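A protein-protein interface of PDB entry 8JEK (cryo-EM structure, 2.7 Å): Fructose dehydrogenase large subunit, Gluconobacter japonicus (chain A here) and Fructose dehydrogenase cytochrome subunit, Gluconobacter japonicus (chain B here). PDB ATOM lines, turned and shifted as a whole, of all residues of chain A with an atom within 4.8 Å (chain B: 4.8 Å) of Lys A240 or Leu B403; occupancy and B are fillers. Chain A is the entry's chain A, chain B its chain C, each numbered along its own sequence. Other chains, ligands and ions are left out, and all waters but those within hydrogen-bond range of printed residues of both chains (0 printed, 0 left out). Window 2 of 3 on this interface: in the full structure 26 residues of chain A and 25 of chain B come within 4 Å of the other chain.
Printed residues of chain B within 4 Å of Asp A211: Leu B403 (3.8 Å). Of the printed residues of chain B, Tyr A236 touches Leu B403 (3.1 Å). Ala A238 touches none of the printed residues of chain B. Of the printed residues of chain B, Ile A239 touches Leu B403 (3.7 Å). Of chain B, only Leu B403 comes within 4 Å of Lys A240. Leu B403 touches four residues of chain A. Printed residues of chain A within 4 Å of Val B404: Arg A44. Printed residues of chain A within 4 Å of Gln B405: Arg A44. The nearest printed residue of chain B that does not touch Lys A240 is Ser B402 (7.6 Å). The nearest residue of chain A that does not touch Leu B403 is Arg A44 (4.3 Å). The nearest printed residue of chain A that does not touch Val B404 is Arg A213 (4.2 Å).
Among the printed residues, pairs that only touch across the chains: Asp A211 with Leu B403, Tyr A236 with Leu B403, Ile A239 with Leu B403 and Lys A240 with Leu B403.
Of the 14 printed residues of chain A, 6 touch a printed residue of chain B. Printed residues of chain A that touch a printed residue of chain B: Arg A44, Asp A211, Tyr A236, Ile A239, Lys A240 and Lys A243. Hydrophobic or aromatic side chains of chain A that line the printed part of chain B: Tyr A236 and Ile A239. Hydrophobic or aromatic side chains of chain B that line the printed part of chain A: Leu B403 and Val B404. Among the printed residues, 7 pairs touch across the chains. Among the printed residues, Asp or Glu carboxylates within 4 Å of a Lys or Arg side-chain nitrogen of the other chain: Lys A243 with Asp B401 (2.7 Å).
OD2 of Asp A211 lies within salt-bridge range of NE of Arg A213 (3.6 Å). The side-chain amino group (NZ) of Lys A240 lies within salt-bridge range of the side-chain carboxylate (OD1) of Asp A211 (2.8 Å). N of Val B404 is in hydrogen-bond range of OG of Ser B402 (3.5 Å). OH of Tyr A236 sits at hydrogen-bond distance from NH2 of Arg A44 (3.0 Å). The side-chain hydroxyl (OG) of Ser B402 is in hydrogen-bond range of the backbone NH (N) of Gln B405.
The backbone carbonyl oxygen (O) of Val B404 lies within hydrogen-bond range of the guanidinium group (NE) of Arg A44, 2.9 Å away. NZ of Lys A243 is in salt-bridge range of OD1 of Asp B401 (2.7 Å). N of Arg A44 lies within hydrogen-bond range of OE1 of Gln B405 (3.1 Å).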
ATOM      1  N   HIS A  24      16.284   8.200 -18.594  1.00  0.00           N
ATOM      2  CA  HIS A  24      16.821   8.803 -17.380  1.00  0.00           C
ATOM      3  C   HIS A  24      15.879   9.862 -16.828  1.00  0.00           C
ATOM      4  O   HIS A  24      15.613   9.898 -15.619  1.00  0.00           O
ATOM      5  CB  HIS A  24      18.199   9.399 -17.668  1.00  0.00           C
ATOM      6  CG  HIS A  24      18.898   9.929 -16.455  1.00  0.00           C
ATOM      7  ND1 HIS A  24      19.777  10.987 -16.506  1.00  0.00           N
ATOM      8  CD2 HIS A  24      18.850   9.542 -15.159  1.00  0.00           C
ATOM      9  CE1 HIS A  24      20.239  11.232 -15.295  1.00  0.00           C
ATOM     10  NE2 HIS A  24      19.693  10.370 -14.458  1.00  0.00           N
ATOM     11  N   ARG A  44      34.052   0.641 -23.521  1.00  0.00           N
ATOM     12  CA  ARG A  44      34.852   1.700 -24.126  1.00  0.00           C
ATOM     13  C   ARG A  44      36.283   1.242 -24.368  1.00  0.00           C
ATOM     14  O   ARG A  44      36.852   1.493 -25.436  1.00  0.00           O
ATOM     15  CB  ARG A  44      34.832   2.939 -23.233  1.00  0.00           C
ATOM     16  CG  ARG A  44      35.988   3.886 -23.456  1.00  0.00           C
ATOM     17  CD  ARG A  44      35.878   5.089 -22.548  1.00  0.00           C
ATOM     18  NE  ARG A  44      34.489   5.410 -22.248  1.00  0.00           N
ATOM     19  CZ  ARG A  44      33.777   6.325 -22.887  1.00  0.00           C
ATOM     20  NH1 ARG A  44      34.295   7.042 -23.869  1.00  0.00           N
ATOM     21  NH2 ARG A  44      32.511   6.524 -22.533  1.00  0.00           N
ATOM     22  N   GLU A 152      23.047  18.491 -19.035  1.00  0.00           N
ATOM     23  CA  GLU A 152      23.166  17.055 -18.801  1.00  0.00           C
ATOM     24  C   GLU A 152      24.392  16.476 -19.499  1.00  0.00           C
ATOM     25  O   GLU A 152      25.098  15.636 -18.930  1.00  0.00           O
ATOM     26  CB  GLU A 152      21.895  16.348 -19.265  1.00  0.00           C
ATOM     27  CG  GLU A 152      22.068  14.870 -19.546  1.00  0.00           C
ATOM     28  CD  GLU A 152      21.644  13.997 -18.385  1.00  0.00           C
ATOM     29  OE1 GLU A 152      21.145  14.544 -17.380  1.00  0.00           O
ATOM     30  OE2 GLU A 152      21.804  12.761 -18.479  1.00  0.00           O
ATOM     31  N   ASP A 211      31.006  16.178 -14.403  1.00  0.00           N
ATOM     32  CA  ASP A 211      30.189  14.969 -14.304  1.00  0.00           C
ATOM     33  C   ASP A 211      31.002  13.761 -13.844  1.00  0.00           C
ATOM     34  O   ASP A 211      30.694  12.623 -14.199  1.00  0.00           O
ATOM     35  CB  ASP A 211      29.487  14.666 -15.633  1.00  0.00           C
ATOM     36  CG  ASP A 211      28.337  13.691 -15.481  1.00  0.00           C
ATOM     37  OD1 ASP A 211      27.798  13.576 -14.361  1.00  0.00           O
ATOM     38  OD2 ASP A 211      27.976  13.037 -16.482  1.00  0.00           O
ATOM     39  N   ARG A 213      33.943  13.019 -14.792  1.00  0.00           N
ATOM     40  CA  ARG A 213      34.727  12.569 -15.924  1.00  0.00           C
ATOM     41  C   ARG A 213      35.900  13.512 -16.158  1.00  0.00           C
ATOM     42  O   ARG A 213      35.830  14.693 -15.803  1.00  0.00           O
ATOM     43  CB  ARG A 213      33.857  12.492 -17.184  1.00  0.00           C
ATOM     44  CG  ARG A 213      32.758  11.447 -17.096  1.00  0.00           C
ATOM     45  CD  ARG A 213      31.916  11.439 -18.348  1.00  0.00           C
ATOM     46  NE  ARG A 213      30.948  12.526 -18.369  1.00  0.00           N
ATOM     47  CZ  ARG A 213      30.908  13.476 -19.293  1.00  0.00           C
ATOM     48  NH1 ARG A 213      31.791  13.522 -20.275  1.00  0.00           N
ATOM     49  NH2 ARG A 213      29.962  14.406 -19.227  1.00  0.00           N
ATOM     50  N   TYR A 236      26.364   7.072 -21.063  1.00  0.00           N
ATOM     51  CA  TYR A 236      26.295   7.718 -19.755  1.00  0.00           C
ATOM     52  C   TYR A 236      24.856   7.830 -19.277  1.00  0.00           C
ATOM     53  O   TYR A 236      24.547   7.504 -18.125  1.00  0.00           O
ATOM     54  CB  TYR A 236      26.927   9.108 -19.807  1.00  0.00           C
ATOM     55  CG  TYR A 236      28.374   9.139 -20.226  1.00  0.00           C
ATOM     56  CD1 TYR A 236      29.194   8.035 -20.060  1.00  0.00           C
ATOM     57  CD2 TYR A 236      28.920  10.281 -20.786  1.00  0.00           C
ATOM     58  CE1 TYR A 236      30.515   8.070 -20.445  1.00  0.00           C
ATOM     59  CE2 TYR A 236      30.234  10.322 -21.172  1.00  0.00           C
ATOM     60  CZ  TYR A 236      31.028   9.217 -20.998  1.00  0.00           C
ATOM     61  OH  TYR A 236      32.343   9.262 -21.385  1.00  0.00           O
ATOM     62  N   ALA A 237      23.964   8.294 -20.152  1.00  0.00           N
ATOM     63  CA  ALA A 237      22.554   8.389 -19.795  1.00  0.00           C
ATOM     64  C   ALA A 237      21.957   7.013 -19.552  1.00  0.00           C
ATOM     65  O   ALA A 237      21.137   6.841 -18.645  1.00  0.00           O
ATOM     66  CB  ALA A 237      21.784   9.128 -20.886  1.00  0.00           C
ATOM     67  N   ALA A 238      22.357   6.017 -20.349  1.00  0.00           N
ATOM     68  CA  ALA A 238      21.867   4.660 -20.120  1.00  0.00           C
ATOM     69  C   ALA A 238      22.303   4.131 -18.756  1.00  0.00           C
ATOM     70  O   ALA A 238      21.503   3.526 -18.031  1.00  0.00           O
ATOM     71  CB  ALA A 238      22.347   3.731 -21.233  1.00  0.00           C
ATOM     72  N   ILE A 239      23.565   4.357 -18.387  1.00  0.00           N
ATOM     73  CA  ILE A 239      24.078   3.900 -17.099  1.00  0.00           C
ATOM     74  C   ILE A 239      23.356   4.605 -15.959  1.00  0.00           C
ATOM     75  O   ILE A 239      22.964   3.980 -14.966  1.00  0.00           O
ATOM     76  CB  ILE A 239      25.600   4.120 -17.023  1.00  0.00           C
ATOM     77  CG1 ILE A 239      26.335   3.143 -17.940  1.00  0.00           C
ATOM     78  CG2 ILE A 239      26.097   3.987 -15.596  1.00  0.00           C
ATOM     79  CD1 ILE A 239      27.745   3.570 -18.276  1.00  0.00           C
ATOM     80  N   LYS A 240      23.172   5.920 -16.084  1.00  0.00           N
ATOM     81  CA  LYS A 240      22.494   6.673 -15.036  1.00  0.00           C
ATOM     82  C   LYS A 240      21.042   6.236 -14.886  1.00  0.00           C
ATOM     83  O   LYS A 240      20.531   6.145 -13.764  1.00  0.00           O
ATOM     84  CB  LYS A 240      22.581   8.169 -15.327  1.00  0.00           C
ATOM     85  CG  LYS A 240      23.973   8.742 -15.168  1.00  0.00           C
ATOM     86  CD  LYS A 240      23.971  10.243 -15.363  1.00  0.00           C
ATOM     87  CE  LYS A 240      25.380  10.798 -15.352  1.00  0.00           C
ATOM     88  NZ  LYS A 240      25.386  12.258 -15.079  1.00  0.00           N
ATOM     89  N   ALA A 241      20.357   5.972 -16.001  1.00  0.00           N
ATOM     90  CA  ALA A 241      18.981   5.492 -15.932  1.00  0.00           C
ATOM     91  C   ALA A 241      18.906   4.110 -15.296  1.00  0.00           C
ATOM     92  O   ALA A 241      18.030   3.854 -14.463  1.00  0.00           O
ATOM     93  CB  ALA A 241      18.361   5.473 -17.328  1.00  0.00           C
ATOM     94  N   GLU A 242      19.814   3.207 -15.674  1.00  0.00           N
ATOM     95  CA  GLU A 242      19.805   1.867 -15.099  1.00  0.00           C
ATOM     96  C   GLU A 242      20.114   1.893 -13.609  1.00  0.00           C
ATOM     97  O   GLU A 242      19.571   1.086 -12.848  1.00  0.00           O
ATOM     98  CB  GLU A 242      20.802   0.974 -15.833  1.00  0.00           C
ATOM     99  CG  GLU A 242      20.629  -0.504 -15.552  1.00  0.00           C
ATOM    100  CD  GLU A 242      21.556  -1.362 -16.385  1.00  0.00           C
ATOM    101  OE1 GLU A 242      22.439  -0.798 -17.064  1.00  0.00           O
ATOM    102  OE2 GLU A 242      21.401  -2.601 -16.365  1.00  0.00           O
ATOM    103  N   LYS A 243      20.989   2.804 -13.175  1.00  0.00           N
ATOM    104  CA  LYS A 243      21.271   2.951 -11.752  1.00  0.00           C
ATOM    105  C   LYS A 243      20.043   3.389 -10.965  1.00  0.00           C
ATOM    106  O   LYS A 243      19.951   3.103  -9.766  1.00  0.00           O
ATOM    107  CB  LYS A 243      22.413   3.951 -11.552  1.00  0.00           C
ATOM    108  CG  LYS A 243      22.862   4.124 -10.113  1.00  0.00           C
ATOM    109  CD  LYS A 243      23.608   2.900  -9.618  1.00  0.00           C
ATOM    110  CE  LYS A 243      23.930   3.013  -8.140  1.00  0.00           C
ATOM    111  NZ  LYS A 243      24.969   2.034  -7.726  1.00  0.00           N
ATOM    112  N   LEU A 244      19.092   4.057 -11.612  1.00  0.00           N
ATOM    113  CA  LEU A 244      17.897   4.562 -10.954  1.00  0.00           C
ATOM    114  C   LEU A 244      16.727   3.588 -11.017  1.00  0.00           C
ATOM    115  O   LEU A 244      15.623   3.938 -10.588  1.00  0.00           O
ATOM    116  CB  LEU A 244      17.491   5.904 -11.562  1.00  0.00           C
ATOM    117  CG  LEU A 244      18.268   7.116 -11.052  1.00  0.00           C
ATOM    118  CD1 LEU A 244      17.666   8.397 -11.587  1.00  0.00           C
ATOM    119  CD2 LEU A 244      18.298   7.130  -9.538  1.00  0.00           C
ATOM    120  N   ASP B 401      30.245   1.422 -10.420  1.00  0.00           N
ATOM    121  CA  ASP B 401      29.439   2.591 -10.740  1.00  0.00           C
ATOM    122  C   ASP B 401      30.122   3.526 -11.729  1.00  0.00           C
ATOM    123  O   ASP B 401      29.656   4.655 -11.918  1.00  0.00           O
ATOM    124  CB  ASP B 401      29.092   3.355  -9.461  1.00  0.00           C
ATOM    125  CG  ASP B 401      28.641   2.441  -8.341  1.00  0.00           C
ATOM    126  OD1 ASP B 401      27.522   1.896  -8.432  1.00  0.00           O
ATOM    127  OD2 ASP B 401      29.403   2.272  -7.368  1.00  0.00           O
ATOM    128  N   SER B 402      31.212   3.087 -12.352  1.00  0.00           N
ATOM    129  CA  SER B 402      31.952   3.937 -13.273  1.00  0.00           C
ATOM    130  C   SER B 402      31.107   4.303 -14.486  1.00  0.00           C
ATOM    131  O   SER B 402      30.289   3.516 -14.967  1.00  0.00           O
ATOM    132  CB  SER B 402      33.230   3.236 -13.727  1.00  0.00           C
ATOM    133  OG  SER B 402      34.115   4.145 -14.353  1.00  0.00           O
ATOM    134  N   LEU B 403      31.311   5.526 -14.976  1.00  0.00           N
ATOM    135  CA  LEU B 403      30.710   5.981 -16.221  1.00  0.00           C
ATOM    136  C   LEU B 403      31.614   5.788 -17.427  1.00  0.00           C
ATOM    137  O   LEU B 403      31.109   5.695 -18.550  1.00  0.00           O
ATOM    138  CB  LEU B 403      30.334   7.464 -16.120  1.00  0.00           C
ATOM    139  CG  LEU B 403      28.860   7.849 -16.238  1.00  0.00           C
ATOM    140  CD1 LEU B 403      28.022   7.146 -15.188  1.00  0.00           C
ATOM    141  CD2 LEU B 403      28.708   9.353 -16.129  1.00  0.00           C
ATOM    142  N   VAL B 404      32.924   5.714 -17.225  1.00  0.00           N
ATOM    143  CA  VAL B 404      33.886   5.616 -18.317  1.00  0.00           C
ATOM    144  C   VAL B 404      34.181   4.167 -18.675  1.00  0.00           C
ATOM    145  O   VAL B 404      34.119   3.784 -19.842  1.00  0.00           O
ATOM    146  CB  VAL B 404      35.180   6.379 -17.953  1.00  0.00           C
ATOM    147  CG1 VAL B 404      36.221   6.208 -19.042  1.00  0.00           C
ATOM    148  CG2 VAL B 404      34.880   7.846 -17.722  1.00  0.00           C
ATOM    149  N   GLN B 405      34.508   3.348 -17.684  1.00  0.00           N
ATOM    150  CA  GLN B 405      34.766   1.935 -17.917  1.00  0.00           C
ATOM    151  C   GLN B 405      34.560   1.151 -16.627  1.00  0.00           C
ATOM    152  O   GLN B 405      35.486   1.036 -15.815  1.00  0.00           O
ATOM    153  CB  GLN B 405      36.180   1.722 -18.455  1.00  0.00           C
ATOM    154  CG  GLN B 405      36.522   0.271 -18.747  1.00  0.00           C
ATOM    155  CD  GLN B 405      35.466  -0.427 -19.576  1.00  0.00           C
ATOM    156  OE1 GLN B 405      35.286  -0.126 -20.752  1.00  0.00           O
ATOM    157  NE2 GLN B 405      34.763  -1.370 -18.964  1.00  0.00           N
